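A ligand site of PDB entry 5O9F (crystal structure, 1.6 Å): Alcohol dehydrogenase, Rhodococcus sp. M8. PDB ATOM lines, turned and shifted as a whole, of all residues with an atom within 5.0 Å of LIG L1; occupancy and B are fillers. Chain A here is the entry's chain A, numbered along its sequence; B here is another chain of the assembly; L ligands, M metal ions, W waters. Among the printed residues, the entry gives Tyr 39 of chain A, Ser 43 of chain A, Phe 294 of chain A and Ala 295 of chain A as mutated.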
ATOM      1  N   CYS A  38      -6.184 -13.638  -9.560  1.00  0.00           N
ATOM      2  CA  CYS A  38      -7.400 -13.103 -10.218  1.00  0.00           C
ATOM      3  C   CYS A  38      -7.964 -14.196 -11.118  1.00  0.00           C
ATOM      4  O   CYS A  38      -7.226 -14.950 -11.728  1.00  0.00           O
ATOM      5  CB  CYS A  38      -7.051 -11.876 -11.056  1.00  0.00           C
ATOM      6  SG  CYS A  38      -8.465 -11.168 -11.938  1.00  0.00           S
ATOM      7  N   TYR A  39      -9.298 -14.291 -11.228  1.00  0.00           N
ATOM      8  CA  TYR A  39      -9.884 -15.318 -12.087  1.00  0.00           C
ATOM      9  C   TYR A  39      -9.459 -15.173 -13.546  1.00  0.00           C
ATOM     10  O   TYR A  39      -9.404 -16.173 -14.282  1.00  0.00           O
ATOM     11  CB  TYR A  39     -11.408 -15.405 -11.917  1.00  0.00           C
ATOM     12  CG  TYR A  39     -11.955 -16.660 -12.548  1.00  0.00           C
ATOM     13  CD1 TYR A  39     -12.341 -16.650 -13.872  1.00  0.00           C
ATOM     14  CD2 TYR A  39     -12.019 -17.863 -11.837  1.00  0.00           C
ATOM     15  CE1 TYR A  39     -12.829 -17.803 -14.477  1.00  0.00           C
ATOM     16  CE2 TYR A  39     -12.492 -19.015 -12.452  1.00  0.00           C
ATOM     17  CZ  TYR A  39     -12.879 -18.968 -13.777  1.00  0.00           C
ATOM     18  OH  TYR A  39     -13.351 -20.102 -14.379  1.00  0.00           O
ATOM     19  N   SER A  40      -9.086 -13.967 -13.963  1.00  0.00           N
ATOM     20  CA  SER A  40      -8.549 -13.807 -15.313  1.00  0.00           C
ATOM     21  C   SER A  40      -7.328 -14.702 -15.559  1.00  0.00           C
ATOM     22  O   SER A  40      -7.103 -15.129 -16.682  1.00  0.00           O
ATOM     23  CB  SER A  40      -8.164 -12.350 -15.590  1.00  0.00           C
ATOM     24  OG  SER A  40      -9.291 -11.489 -15.571  1.00  0.00           O
ATOM     25  N   SER A  43      -8.647 -17.941 -16.902  1.00  0.00           N
ATOM     26  CA  SER A  43      -9.017 -17.780 -18.318  1.00  0.00           C
ATOM     27  C   SER A  43      -7.787 -17.741 -19.228  1.00  0.00           C
ATOM     28  O   SER A  43      -7.786 -18.368 -20.281  1.00  0.00           O
ATOM     29  CB  SER A  43      -9.895 -16.536 -18.510  1.00  0.00           C
ATOM     30  OG  SER A  43     -11.057 -16.633 -17.725  1.00  0.00           O
ATOM     31  N   ASP A 153      -6.570  -4.708  -8.555  1.00  0.00           N
ATOM     32  CA  ASP A 153      -7.442  -5.148  -9.646  1.00  0.00           C
ATOM     33  C   ASP A 153      -8.856  -5.456  -9.137  1.00  0.00           C
ATOM     34  O   ASP A 153      -9.819  -4.876  -9.639  1.00  0.00           O
ATOM     35  CB  ASP A 153      -6.825  -6.343 -10.354  1.00  0.00           C
ATOM     36  CG  ASP A 153      -7.415  -6.602 -11.711  1.00  0.00           C
ATOM     37  OD1 ASP A 153      -8.024  -5.703 -12.356  1.00  0.00           O
ATOM     38  OD2 ASP A 153      -7.166  -7.733 -12.149  1.00  0.00           O
ATOM     39  N   THR A 157     -10.769  -2.340 -10.679  1.00  0.00           N
ATOM     40  CA  THR A 157     -11.645  -2.582 -11.810  1.00  0.00           C
ATOM     41  C   THR A 157     -13.108  -2.231 -11.456  1.00  0.00           C
ATOM     42  O   THR A 157     -13.735  -1.466 -12.190  1.00  0.00           O
ATOM     43  CB  THR A 157     -11.453  -3.998 -12.344  1.00  0.00           C
ATOM     44  OG1 THR A 157     -10.133  -4.065 -12.891  1.00  0.00           O
ATOM     45  CG2 THR A 157     -12.474  -4.335 -13.410  1.00  0.00           C
ATOM     46  N   ILE A 178     -23.684  -8.359  -9.731  1.00  0.00           N
ATOM     47  CA  ILE A 178     -23.780  -9.777 -10.051  1.00  0.00           C
ATOM     48  C   ILE A 178     -22.406 -10.412  -9.928  1.00  0.00           C
ATOM     49  O   ILE A 178     -21.474 -10.035 -10.633  1.00  0.00           O
ATOM     50  CB  ILE A 178     -24.357 -10.049 -11.438  1.00  0.00           C
ATOM     51  CG1 ILE A 178     -25.663  -9.267 -11.671  1.00  0.00           C
ATOM     52  CG2 ILE A 178     -24.573 -11.550 -11.611  1.00  0.00           C
ATOM     53  CD1 ILE A 178     -26.260  -9.475 -13.056  1.00  0.00           C
ATOM     54  N   GLY A 179     -22.279 -11.376  -9.015  1.00  0.00           N
ATOM     55  CA  GLY A 179     -21.025 -12.087  -8.754  1.00  0.00           C
ATOM     56  C   GLY A 179     -20.331 -11.498  -7.554  1.00  0.00           C
ATOM     57  O   GLY A 179     -19.745 -10.430  -7.686  1.00  0.00           O
ATOM     58  N   VAL A 180     -20.408 -12.166  -6.414  1.00  0.00           N
ATOM     59  CA  VAL A 180     -19.811 -11.684  -5.152  1.00  0.00           C
ATOM     60  C   VAL A 180     -18.530 -12.473  -4.866  1.00  0.00           C
ATOM     61  O   VAL A 180     -18.420 -13.229  -3.892  1.00  0.00           O
ATOM     62  CB  VAL A 180     -20.806 -11.760  -3.985  1.00  0.00           C
ATOM     63  CG1 VAL A 180     -20.251 -11.027  -2.757  1.00  0.00           C
ATOM     64  CG2 VAL A 180     -22.129 -11.141  -4.422  1.00  0.00           C
ATOM     65  N   GLY A 181     -17.577 -12.324  -5.764  1.00  0.00           N
ATOM     66  CA  GLY A 181     -16.257 -12.957  -5.647  1.00  0.00           C
ATOM     67  C   GLY A 181     -15.210 -11.925  -5.314  1.00  0.00           C
ATOM     68  O   GLY A 181     -15.485 -10.962  -4.569  1.00  0.00           O
ATOM     69  N   GLY A 182     -13.994 -12.111  -5.832  1.00  0.00           N
ATOM     70  CA  GLY A 182     -12.928 -11.153  -5.591  1.00  0.00           C
ATOM     71  C   GLY A 182     -13.331  -9.712  -5.919  1.00  0.00           C
ATOM     72  O   GLY A 182     -13.281  -8.840  -5.048  1.00  0.00           O
ATOM     73  N   LEU A 183     -13.767  -9.492  -7.149  1.00  0.00           N
ATOM     74  CA  LEU A 183     -14.171  -8.154  -7.580  1.00  0.00           C
ATOM     75  C   LEU A 183     -15.481  -7.738  -6.912  1.00  0.00           C
ATOM     76  O   LEU A 183     -15.582  -6.635  -6.367  1.00  0.00           O
ATOM     77  CB  LEU A 183     -14.342  -8.090  -9.117  1.00  0.00           C
ATOM     78  CG  LEU A 183     -13.123  -7.694  -9.917  1.00  0.00           C
ATOM     79  CD1 LEU A 183     -12.022  -8.739  -9.856  1.00  0.00           C
ATOM     80  CD2 LEU A 183     -13.488  -7.381 -11.354  1.00  0.00           C
ATOM     81  N   GLY A 184     -16.481  -8.607  -6.967  1.00  0.00           N
ATOM     82  CA  GLY A 184     -17.822  -8.222  -6.551  1.00  0.00           C
ATOM     83  C   GLY A 184     -17.951  -7.823  -5.087  1.00  0.00           C
ATOM     84  O   GLY A 184     -18.690  -6.884  -4.752  1.00  0.00           O
ATOM     85  N   VAL A 202     -26.172 -10.402  -6.192  1.00  0.00           N
ATOM     86  CA  VAL A 202     -26.699 -11.610  -6.862  1.00  0.00           C
ATOM     87  C   VAL A 202     -25.544 -12.623  -6.965  1.00  0.00           C
ATOM     88  O   VAL A 202     -24.462 -12.275  -7.430  1.00  0.00           O
ATOM     89  CB  VAL A 202     -27.213 -11.256  -8.280  1.00  0.00           C
ATOM     90  CG1 VAL A 202     -27.749 -12.481  -8.973  1.00  0.00           C
ATOM     91  CG2 VAL A 202     -28.283 -10.150  -8.225  1.00  0.00           C
ATOM     92  N   ASP A 203     -25.780 -13.852  -6.545  1.00  0.00           N
ATOM     93  CA  ASP A 203     -24.768 -14.915  -6.699  1.00  0.00           C
ATOM     94  C   ASP A 203     -25.469 -16.263  -6.762  1.00  0.00           C
ATOM     95  O   ASP A 203     -26.618 -16.405  -6.316  1.00  0.00           O
ATOM     96  CB  ASP A 203     -23.725 -14.870  -5.567  1.00  0.00           C
ATOM     97  CG  ASP A 203     -22.382 -15.504  -5.964  1.00  0.00           C
ATOM     98  OD1 ASP A 203     -22.316 -16.743  -6.135  1.00  0.00           O
ATOM     99  OD2 ASP A 203     -21.400 -14.767  -6.105  1.00  0.00           O
ATOM    100  N   LEU A 204     -24.802 -17.242  -7.348  1.00  0.00           N
ATOM    101  CA  LEU A 204     -25.294 -18.626  -7.348  1.00  0.00           C
ATOM    102  C   LEU A 204     -25.214 -19.302  -5.979  1.00  0.00           C
ATOM    103  O   LEU A 204     -25.984 -20.209  -5.694  1.00  0.00           O
ATOM    104  CB  LEU A 204     -24.497 -19.470  -8.334  1.00  0.00           C
ATOM    105  CG  LEU A 204     -24.731 -19.180  -9.817  1.00  0.00           C
ATOM    106  CD1 LEU A 204     -23.666 -19.905 -10.655  1.00  0.00           C
ATOM    107  CD2 LEU A 204     -26.121 -19.615 -10.251  1.00  0.00           C
ATOM    108  N   ASP A 205     -24.267 -18.855  -5.162  1.00  0.00           N
ATOM    109  CA  ASP A 205     -23.857 -19.556  -3.947  1.00  0.00           C
ATOM    110  C   ASP A 205     -24.404 -18.804  -2.702  1.00  0.00           C
ATOM    111  O   ASP A 205     -24.112 -17.632  -2.528  1.00  0.00           O
ATOM    112  CB  ASP A 205     -22.324 -19.595  -3.958  1.00  0.00           C
ATOM    113  CG  ASP A 205     -21.710 -20.297  -2.765  1.00  0.00           C
ATOM    114  OD1 ASP A 205     -22.362 -20.470  -1.725  1.00  0.00           O
ATOM    115  OD2 ASP A 205     -20.512 -20.680  -2.874  1.00  0.00           O
ATOM    116  N   ARG A 208     -21.948 -16.950  -0.650  1.00  0.00           N
ATOM    117  CA  ARG A 208     -21.554 -15.678  -1.226  1.00  0.00           C
ATOM    118  C   ARG A 208     -22.595 -14.607  -1.023  1.00  0.00           C
ATOM    119  O   ARG A 208     -22.250 -13.434  -0.914  1.00  0.00           O
ATOM    120  CB  ARG A 208     -21.227 -15.821  -2.727  1.00  0.00           C
ATOM    121  CG  ARG A 208     -20.118 -16.781  -3.042  1.00  0.00           C
ATOM    122  CD  ARG A 208     -18.807 -16.426  -2.322  1.00  0.00           C
ATOM    123  NE  ARG A 208     -17.773 -17.438  -2.524  1.00  0.00           N
ATOM    124  CZ  ARG A 208     -16.805 -17.415  -3.453  1.00  0.00           C
ATOM    125  NH1 ARG A 208     -16.599 -16.353  -4.236  1.00  0.00           N
ATOM    126  NH2 ARG A 208     -15.949 -18.457  -3.517  1.00  0.00           N
ATOM    127  N   SER A 223     -28.951 -16.043  -7.994  1.00  0.00           N
ATOM    128  CA  SER A 223     -28.838 -15.894  -9.441  1.00  0.00           C
ATOM    129  C   SER A 223     -29.586 -17.011 -10.152  1.00  0.00           C
ATOM    130  O   SER A 223     -29.967 -17.994  -9.543  1.00  0.00           O
ATOM    131  CB  SER A 223     -27.367 -15.928  -9.876  1.00  0.00           C
ATOM    132  OG  SER A 223     -27.204 -15.389 -11.196  1.00  0.00           O
ATOM    133  N   PHE A 246     -20.183  -8.735 -12.743  1.00  0.00           N
ATOM    134  CA  PHE A 246     -18.822  -9.250 -12.557  1.00  0.00           C
ATOM    135  C   PHE A 246     -18.696 -10.702 -12.955  1.00  0.00           C
ATOM    136  O   PHE A 246     -17.639 -11.301 -12.729  1.00  0.00           O
ATOM    137  CB  PHE A 246     -18.372  -9.030 -11.099  1.00  0.00           C
ATOM    138  CG  PHE A 246     -18.313  -7.588 -10.721  1.00  0.00           C
ATOM    139  CD1 PHE A 246     -17.328  -6.758 -11.232  1.00  0.00           C
ATOM    140  CD2 PHE A 246     -19.289  -7.042  -9.891  1.00  0.00           C
ATOM    141  CE1 PHE A 246     -17.297  -5.402 -10.925  1.00  0.00           C
ATOM    142  CE2 PHE A 246     -19.251  -5.693  -9.563  1.00  0.00           C
ATOM    143  CZ  PHE A 246     -18.276  -4.884 -10.090  1.00  0.00           C
ATOM    144  N   VAL A 247     -19.738 -11.289 -13.550  1.00  0.00           N
ATOM    145  CA  VAL A 247     -19.692 -12.643 -14.098  1.00  0.00           C
ATOM    146  C   VAL A 247     -19.562 -12.541 -15.622  1.00  0.00           C
ATOM    147  O   VAL A 247     -18.624 -13.068 -16.216  1.00  0.00           O
ATOM    148  CB  VAL A 247     -20.948 -13.453 -13.716  1.00  0.00           C
ATOM    149  CG1 VAL A 247     -20.905 -14.882 -14.289  1.00  0.00           C
ATOM    150  CG2 VAL A 247     -21.127 -13.518 -12.211  1.00  0.00           C
ATOM    151  N   SER A 251     -26.142 -15.654 -19.406  1.00  0.00           N
ATOM    152  CA  SER A 251     -27.305 -15.657 -18.500  1.00  0.00           C
ATOM    153  C   SER A 251     -27.348 -14.417 -17.583  1.00  0.00           C
ATOM    154  O   SER A 251     -28.435 -13.860 -17.335  1.00  0.00           O
ATOM    155  CB  SER A 251     -27.357 -16.927 -17.664  1.00  0.00           C
ATOM    156  OG  SER A 251     -26.171 -17.086 -16.922  1.00  0.00           O
ATOM    157  N   THR A 252     -26.204 -13.982 -17.096  1.00  0.00           N
ATOM    158  CA  THR A 252     -26.129 -12.803 -16.215  1.00  0.00           C
ATOM    159  C   THR A 252     -26.338 -11.496 -16.988  1.00  0.00           C
ATOM    160  O   THR A 252     -27.017 -10.591 -16.499  1.00  0.00           O
ATOM    161  CB  THR A 252     -24.830 -12.748 -15.379  1.00  0.00           C
ATOM    162  OG1 THR A 252     -23.699 -12.723 -16.239  1.00  0.00           O
ATOM    163  CG2 THR A 252     -24.745 -13.969 -14.470  1.00  0.00           C
ATOM    164  N   VAL A 269     -18.449  -6.461 -16.766  1.00  0.00           N
ATOM    165  CA  VAL A 269     -17.090  -6.462 -16.235  1.00  0.00           C
ATOM    166  C   VAL A 269     -16.454  -7.835 -16.325  1.00  0.00           C
ATOM    167  O   VAL A 269     -15.294  -7.968 -16.720  1.00  0.00           O
ATOM    168  CB  VAL A 269     -17.042  -5.936 -14.798  1.00  0.00           C
ATOM    169  CG1 VAL A 269     -15.595  -5.856 -14.311  1.00  0.00           C
ATOM    170  CG2 VAL A 269     -17.722  -4.583 -14.690  1.00  0.00           C
ATOM    171  N   GLY A 270     -17.186  -8.863 -15.910  1.00  0.00           N
ATOM    172  CA  GLY A 270     -16.716 -10.240 -16.023  1.00  0.00           C
ATOM    173  C   GLY A 270     -16.551 -10.646 -17.488  1.00  0.00           C
ATOM    174  O   GLY A 270     -17.242 -10.123 -18.375  1.00  0.00           O
ATOM    175  N   ILE A 271     -15.605 -11.539 -17.731  1.00  0.00           N
ATOM    176  CA  ILE A 271     -15.172 -11.908 -19.078  1.00  0.00           C
ATOM    177  C   ILE A 271     -15.487 -13.374 -19.349  1.00  0.00           C
ATOM    178  O   ILE A 271     -14.839 -14.294 -18.808  1.00  0.00           O
ATOM    179  CB  ILE A 271     -13.668 -11.623 -19.302  1.00  0.00           C
ATOM    180  CG1 ILE A 271     -13.346 -10.141 -19.032  1.00  0.00           C
ATOM    181  CG2 ILE A 271     -13.241 -12.043 -20.719  1.00  0.00           C
ATOM    182  CD1 ILE A 271     -11.868  -9.820 -18.865  1.00  0.00           C
ATOM    183  N   PRO A 293     -15.936  -2.214 -19.412  1.00  0.00           N
ATOM    184  CA  PRO A 293     -14.811  -1.399 -18.945  1.00  0.00           C
ATOM    185  C   PRO A 293     -13.576  -2.268 -18.753  1.00  0.00           C
ATOM    186  O   PRO A 293     -13.690  -3.512 -18.699  1.00  0.00           O
ATOM    187  CB  PRO A 293     -15.328  -0.862 -17.632  1.00  0.00           C
ATOM    188  CG  PRO A 293     -16.152  -1.971 -17.089  1.00  0.00           C
ATOM    189  CD  PRO A 293     -16.823  -2.596 -18.297  1.00  0.00           C
ATOM    190  N   PHE A 294     -12.404  -1.651 -18.660  1.00  0.00           N
ATOM    191  CA  PHE A 294     -11.172  -2.407 -18.491  1.00  0.00           C
ATOM    192  C   PHE A 294     -10.280  -1.734 -17.439  1.00  0.00           C
ATOM    193  O   PHE A 294      -9.924  -0.559 -17.603  1.00  0.00           O
ATOM    194  CB  PHE A 294     -10.421  -2.533 -19.796  1.00  0.00           C
ATOM    195  CG  PHE A 294      -9.147  -3.297 -19.686  1.00  0.00           C
ATOM    196  CD1 PHE A 294      -9.179  -4.693 -19.541  1.00  0.00           C
ATOM    197  CD2 PHE A 294      -7.929  -2.647 -19.698  1.00  0.00           C
ATOM    198  CE1 PHE A 294      -7.989  -5.399 -19.428  1.00  0.00           C
ATOM    199  CE2 PHE A 294      -6.741  -3.363 -19.569  1.00  0.00           C
ATOM    200  CZ  PHE A 294      -6.787  -4.730 -19.442  1.00  0.00           C
ATOM    201  N   ALA A 295      -9.946  -2.475 -16.391  1.00  0.00           N
ATOM    202  CA  ALA A 295      -9.034  -2.035 -15.355  1.00  0.00           C
ATOM    203  C   ALA A 295      -9.441  -0.682 -14.805  1.00  0.00           C
ATOM    204  O   ALA A 295     -10.635  -0.473 -14.545  1.00  0.00           O
ATOM    205  CB  ALA A 295      -7.594  -2.074 -15.893  1.00  0.00           C
ATOM    206  N   LEU A 332      -9.053 -21.499  -6.689  1.00  0.00           N
ATOM    207  CA  LEU A 332      -9.734 -20.453  -7.451  1.00  0.00           C
ATOM    208  C   LEU A 332     -10.587 -21.063  -8.578  1.00  0.00           C
ATOM    209  O   LEU A 332     -11.763 -20.702  -8.756  1.00  0.00           O
ATOM    210  CB  LEU A 332      -8.738 -19.443  -8.025  1.00  0.00           C
ATOM    211  CG  LEU A 332      -9.303 -18.243  -8.781  1.00  0.00           C
ATOM    212  CD1 LEU A 332     -10.292 -17.472  -7.915  1.00  0.00           C
ATOM    213  CD2 LEU A 332      -8.151 -17.358  -9.248  1.00  0.00           C
ATOM    214  N   GLY A 339     -13.597 -14.806  -1.249  1.00  0.00           N
ATOM    215  CA  GLY A 339     -12.989 -13.510  -1.495  1.00  0.00           C
ATOM    216  C   GLY A 339     -11.810 -13.664  -2.440  1.00  0.00           C
ATOM    217  O   GLY A 339     -11.938 -14.284  -3.505  1.00  0.00           O
ATOM    218  N   ARG A 340     -10.652 -13.108  -2.041  1.00  0.00           N
ATOM    219  CA  ARG A 340      -9.431 -13.129  -2.834  1.00  0.00           C
ATOM    220  C   ARG A 340      -8.340 -14.009  -2.248  1.00  0.00           C
ATOM    221  O   ARG A 340      -8.028 -13.910  -1.066  1.00  0.00           O
ATOM    222  CB  ARG A 340      -8.890 -11.695  -2.964  1.00  0.00           C
ATOM    223  CG  ARG A 340      -9.134 -11.053  -4.304  1.00  0.00           C
ATOM    224  CD  ARG A 340      -8.225 -11.621  -5.348  1.00  0.00           C
ATOM    225  NE  ARG A 340      -8.241 -10.814  -6.564  1.00  0.00           N
ATOM    226  CZ  ARG A 340      -9.031 -10.981  -7.623  1.00  0.00           C
ATOM    227  NH1 ARG A 340      -9.976 -11.914  -7.652  1.00  0.00           N
ATOM    228  NH2 ARG A 340      -8.885 -10.179  -8.655  1.00  0.00           N
ATOM    229  N   PHE B 281     -16.810  -8.560 -24.521  1.00  0.00           N
ATOM    230  CA  PHE B 281     -15.368  -8.638 -24.689  1.00  0.00           C
ATOM    231  C   PHE B 281     -15.013  -9.330 -26.003  1.00  0.00           C
ATOM    232  O   PHE B 281     -15.716 -10.259 -26.418  1.00  0.00           O
ATOM    233  CB  PHE B 281     -14.734  -9.329 -23.499  1.00  0.00           C
ATOM    234  CG  PHE B 281     -14.746  -8.466 -22.258  1.00  0.00           C
ATOM    235  CD1 PHE B 281     -13.768  -7.482 -22.072  1.00  0.00           C
ATOM    236  CD2 PHE B 281     -15.786  -8.572 -21.332  1.00  0.00           C
ATOM    237  CE1 PHE B 281     -13.818  -6.653 -20.954  1.00  0.00           C
ATOM    238  CE2 PHE B 281     -15.831  -7.746 -20.227  1.00  0.00           C
ATOM    239  CZ  PHE B 281     -14.848  -6.794 -20.025  1.00  0.00           C
HETATM  240  P1  LIG L   1     -14.037 -15.058  -8.669  1.00  0.00           P
HETATM  241  O1  LIG L   1     -13.891 -16.470  -9.206  1.00  0.00           O
HETATM  242  O2  LIG L   1     -13.337 -14.562  -7.432  1.00  0.00           O
HETATM  243  O3  LIG L   1     -15.592 -14.772  -8.345  1.00  0.00           O
HETATM  244  C1  LIG L   1     -16.664 -15.342  -9.102  1.00  0.00           C
HETATM  245  C2  LIG L   1     -17.952 -15.092  -8.347  1.00  0.00           C
HETATM  246  O4  LIG L   1     -19.008 -15.130  -9.309  1.00  0.00           O
HETATM  247  C3  LIG L   1     -18.246 -16.170  -7.310  1.00  0.00           C
HETATM  248  O5  LIG L   1     -18.776 -15.613  -6.106  1.00  0.00           O
HETATM  249  C4  LIG L   1     -19.252 -17.054  -8.010  1.00  0.00           C
HETATM  250  O6  LIG L   1     -20.136 -17.792  -7.186  1.00  0.00           O
HETATM  251  C5  LIG L   1     -20.008 -16.025  -8.829  1.00  0.00           C
HETATM  252  N1  LIG L   1     -20.740 -16.530  -9.991  1.00  0.00           N
HETATM  253  C6  LIG L   1     -20.283 -17.351 -10.957  1.00  0.00           C
HETATM  254  N2  LIG L   1     -21.243 -17.562 -11.887  1.00  0.00           N
HETATM  255  C7  LIG L   1     -22.319 -16.843 -11.520  1.00  0.00           C
HETATM  256  C8  LIG L   1     -23.672 -16.582 -12.038  1.00  0.00           C
HETATM  257  N3  LIG L   1     -24.099 -17.175 -13.183  1.00  0.00           N
HETATM  258  N4  LIG L   1     -24.477 -15.749 -11.360  1.00  0.00           N
HETATM  259  C9  LIG L   1     -24.095 -15.157 -10.209  1.00  0.00           C
HETATM  260  N5  LIG L   1     -22.880 -15.349  -9.665  1.00  0.00           N
HETATM  261  C10 LIG L   1     -21.977 -16.155 -10.264  1.00  0.00           C
HETATM  262  O7  LIG L   1     -13.759 -14.050  -9.899  1.00  0.00           O
HETATM  263  P2  LIG L   1     -13.005 -12.608  -9.887  1.00  0.00           P
HETATM  264  O8  LIG L   1     -11.532 -12.824  -9.817  1.00  0.00           O
HETATM  265  O9  LIG L   1     -13.778 -11.726  -8.946  1.00  0.00           O
HETATM  266  O10 LIG L   1     -13.266 -12.229 -11.436  1.00  0.00           O
HETATM  267  C11 LIG L   1     -14.589 -11.953 -11.892  1.00  0.00           C
HETATM  268  C12 LIG L   1     -14.581 -11.759 -13.395  1.00  0.00           C
HETATM  269  O11 LIG L   1     -14.033 -10.453 -13.666  1.00  0.00           O
HETATM  270  C13 LIG L   1     -13.763 -12.746 -14.206  1.00  0.00           C
HETATM  271  O12 LIG L   1     -14.411 -13.028 -15.465  1.00  0.00           O
HETATM  272  C14 LIG L   1     -12.488 -11.994 -14.493  1.00  0.00           C
HETATM  273  O13 LIG L   1     -11.775 -12.464 -15.630  1.00  0.00           O
HETATM  274  C15 LIG L   1     -13.060 -10.593 -14.699  1.00  0.00           C
HETATM  275  N6  LIG L   1     -12.142  -9.451 -14.575  1.00  0.00           N
HETATM  276  C16 LIG L   1     -12.293  -8.432 -15.431  1.00  0.00           C
HETATM  277  C17 LIG L   1     -11.528  -7.284 -15.381  1.00  0.00           C
HETATM  278  C18 LIG L   1     -11.733  -6.168 -16.361  1.00  0.00           C
HETATM  279  O14 LIG L   1     -10.857  -5.319 -16.480  1.00  0.00           O
HETATM  280  N7  LIG L   1     -12.910  -6.038 -17.002  1.00  0.00           N
HETATM  281  C19 LIG L   1     -10.529  -7.184 -14.399  1.00  0.00           C
HETATM  282  C20 LIG L   1     -10.439  -8.226 -13.469  1.00  0.00           C
HETATM  283  C21 LIG L   1     -11.239  -9.350 -13.568  1.00  0.00           C
HETATM  284  O1  LG2 L   2      -8.835  -9.661 -20.883  1.00  0.00           O
HETATM  285  C1  LG2 L   2      -7.722  -9.478 -20.336  1.00  0.00           C
HETATM  286  O2  LG2 L   2      -6.964  -8.522 -20.627  1.00  0.00           O
HETATM  287  C2  LG2 L   2      -7.268 -10.485 -19.313  1.00  0.00           C
HETATM  288  C3  LG2 L   2      -6.253 -11.412 -19.977  1.00  0.00           C
HETATM  289  C4  LG2 L   2      -6.678  -9.803 -18.078  1.00  0.00           C
HETATM  290  C5  LG2 L   2      -7.724  -8.989 -17.311  1.00  0.00           C
HETATM  291  C6  LG2 L   2      -7.215  -8.677 -15.918  1.00  0.00           C
HETATM  292  O3  LG2 L   2      -6.374  -7.756 -15.826  1.00  0.00           O
HETATM  293  O4  LG2 L   2      -7.656  -9.321 -14.929  1.00  0.00           O
HETATM  294 ZN    ZN M   1      -7.278  -9.487 -13.024  1.00  0.00          ZN
HETATM  295  O   HOH W   1     -15.165 -16.993 -11.624  1.00  0.00           O
HETATM  296  O   HOH W   2     -13.686 -18.800  -8.042  1.00  0.00           O
HETATM  297  O   HOH W   3     -20.825 -20.389  -7.962  1.00  0.00           O
HETATM  298  O   HOH W   4     -17.976 -12.490 -10.295  1.00  0.00           O
HETATM  299  O   HOH W   5     -17.200 -18.701 -10.831  1.00  0.00           O
HETATM  300  O   HOH W   6     -12.378 -14.474 -17.356  1.00  0.00           O
HETATM  301  O   HOH W   7     -11.026 -14.185  -6.069  1.00  0.00           O
HETATM  302  O   HOH W   8     -26.832 -17.045 -14.283  1.00  0.00           O
HETATM  303  O   HOH W   9     -22.764 -19.302 -14.752  1.00  0.00           O
HETATM  304  O   HOH W  10     -20.346 -19.242 -13.832  1.00  0.00           O
HETATM  305  O   HOH W  11     -16.584 -14.525 -15.189  1.00  0.00           O
HETATM  306  O   HOH W  12     -13.988 -15.767  -5.060  1.00  0.00           O
HETATM  307  O   HOH W  13     -16.430 -11.148  -8.296  1.00  0.00           O
HETATM  308  O   HOH W  14     -17.586 -19.425  -5.885  1.00  0.00           O
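The guanidinium group of Arg 340 lies within salt-bridge range of an oxygen (O8) of LIG L1, at 2.8 Å.
The backbone NH of Ile 271 sits at hydrogen-bond distance from an oxygen (O12) of LIG L1 (3.0 Å).
The backbone NH (N) of Gly 182 lies within hydrogen-bond range of an oxygen (O2) of LIG L1, at 3.0 Å.
A nitrogen (N7) of LIG L1 is in hydrogen-bond range of the backbone carbonyl oxygen of Pro 293 (3.1 Å).
The backbone NH (N) of Tyr 39 is in hydrogen-bond range of an oxygen (O8) of LIG L1, 3.0 Å away.
O5 of LIG L1 is in hydrogen-bond range of NH1 of Arg 208, at 3.0 Å.
An oxygen (O6) of LIG L1 sits at hydrogen-bond distance from the side-chain carboxylate of Asp 203 (2.6 Å).
An oxygen (O13) of LIG L1 is in hydrogen-bond range of the side-chain hydroxyl (OG) of Ser 40 (2.7 Å).
O4 of LG2 L2 lies close to OG of Ser 40 (2.8 Å).
A nitrogen (N7) of LIG L1 sits at hydrogen-bond distance from the backbone carbonyl oxygen of Val 269 (3.1 Å).
N of Ala 295 sits at hydrogen-bond distance from O14 of LIG L1.
An oxygen (O5) of LIG L1 lies within hydrogen-bond range of the backbone carbonyl oxygen of Val 180 (3.3 Å).
N4 of LIG L1 sits at hydrogen-bond distance from OG of Ser 223 (2.8 Å).
The backbone NH of Leu 183 sits at hydrogen-bond distance from an oxygen (O9) of LIG L1 (2.9 Å).
The backbone NH of Ser 40 sits close to the side-chain sulfur of Cys 38 (3.5 Å).
The backbone NH of Asp 205 sits at hydrogen-bond distance from the side-chain carboxylate of Asp 203 (3.0 Å).
NH2 of Arg 340 lies close to SG of Cys 38.
OG1 of Thr 157 sits at hydrogen-bond distance from OD1 of Asp 153 (2.7 Å).
The backbone NH of Gly 179 sits at hydrogen-bond distance from the backbone carbonyl oxygen of Val 202, 2.8 Å away.
The backbone NH (N) of Phe 246 lies within hydrogen-bond range of the backbone carbonyl oxygen (O) of Ile 178, 2.8 Å away.
The backbone carbonyl oxygen of Asp 203 sits at hydrogen-bond distance from the backbone NH of Ser 223, 2.9 Å away.
OD2 of Asp 203 lies within hydrogen-bond range of N of Val 180.
Water W2 bridges O1 of LIG L1 (2.6 Å) and O of Leu 332 (2.8 Å).
Water W11 bridges an oxygen (O12) of LIG L1 and the backbone carbonyl oxygen (O) of Val 247.
Water W7 lies within hydrogen-bond range of an oxygen (O2) of LIG L1 (2.7 Å), the backbone carbonyl oxygen (O) of Gly 339 (2.7 Å) and the guanidinium group (NH1) of Arg 340 (3.0 Å).
Water W6 lies within hydrogen-bond range of OG of Ser 43 (2.6 Å), O13 of LIG L1 (2.7 Å) and O of Ile 271 (2.9 Å).
Water W12 lies within hydrogen-bond range of O2 of LIG L1 (2.7 Å), NH1 of Arg 208 (2.8 Å) and O of Gly 339 (3.0 Å).
Water W14 lies within hydrogen-bond range of the guanidinium group (NH2) of Arg 208 and an oxygen (O6) of LIG L1.
SG of Cys 38 touches C21 of LIG L1 (3.7 Å).
Asp 153 touches LIG L1 (OD1 to C19, 3.6 Å).
Thr 157 touches LIG L1.
CG2 of Ile 178 touches C9 of LIG L1, 3.9 Å away.
Gly 179 touches LIG L1 (CA to O4, 3.7 Å).
CA of Gly 181 touches O3 of LIG L1, at 3.3 Å.
Leu 204 touches LIG L1 (CD1 to C7, 3.5 Å).
Phe 246 touches LIG L1.
CG2 of Val 247 touches C10 of LIG L1, at 3.4 Å.
Thr 252 touches LIG L1.
Gly 270 touches LIG L1 (CA to O11, 3.6 Å).
Phe 294 touches LIG L1 (CD1 to O14, 3.5 Å).
Leu 332 touches LIG L1 (CD1 to O1, 3.95 Å).
Phe 281 of chain B touches LIG L1.
27 residues have an atom within 4 Å of LIG L1: Cys 38, Tyr 39, Ser 40, Asp 153, Thr 157, Ile 178, Gly 179, Val 180, Gly 181, Gly 182, Leu 183, Asp 203, Leu 204, Arg 208, Ser 223, Phe 246, Val 247, Thr 252, Val 269, Gly 270, Ile 271, Pro 293, Phe 294, Ala 295, Leu 332, Arg 340 and Phe 281 of chain B.
Along chain A the residues within 4 Å of LIG L1 span positions 38 to 340.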
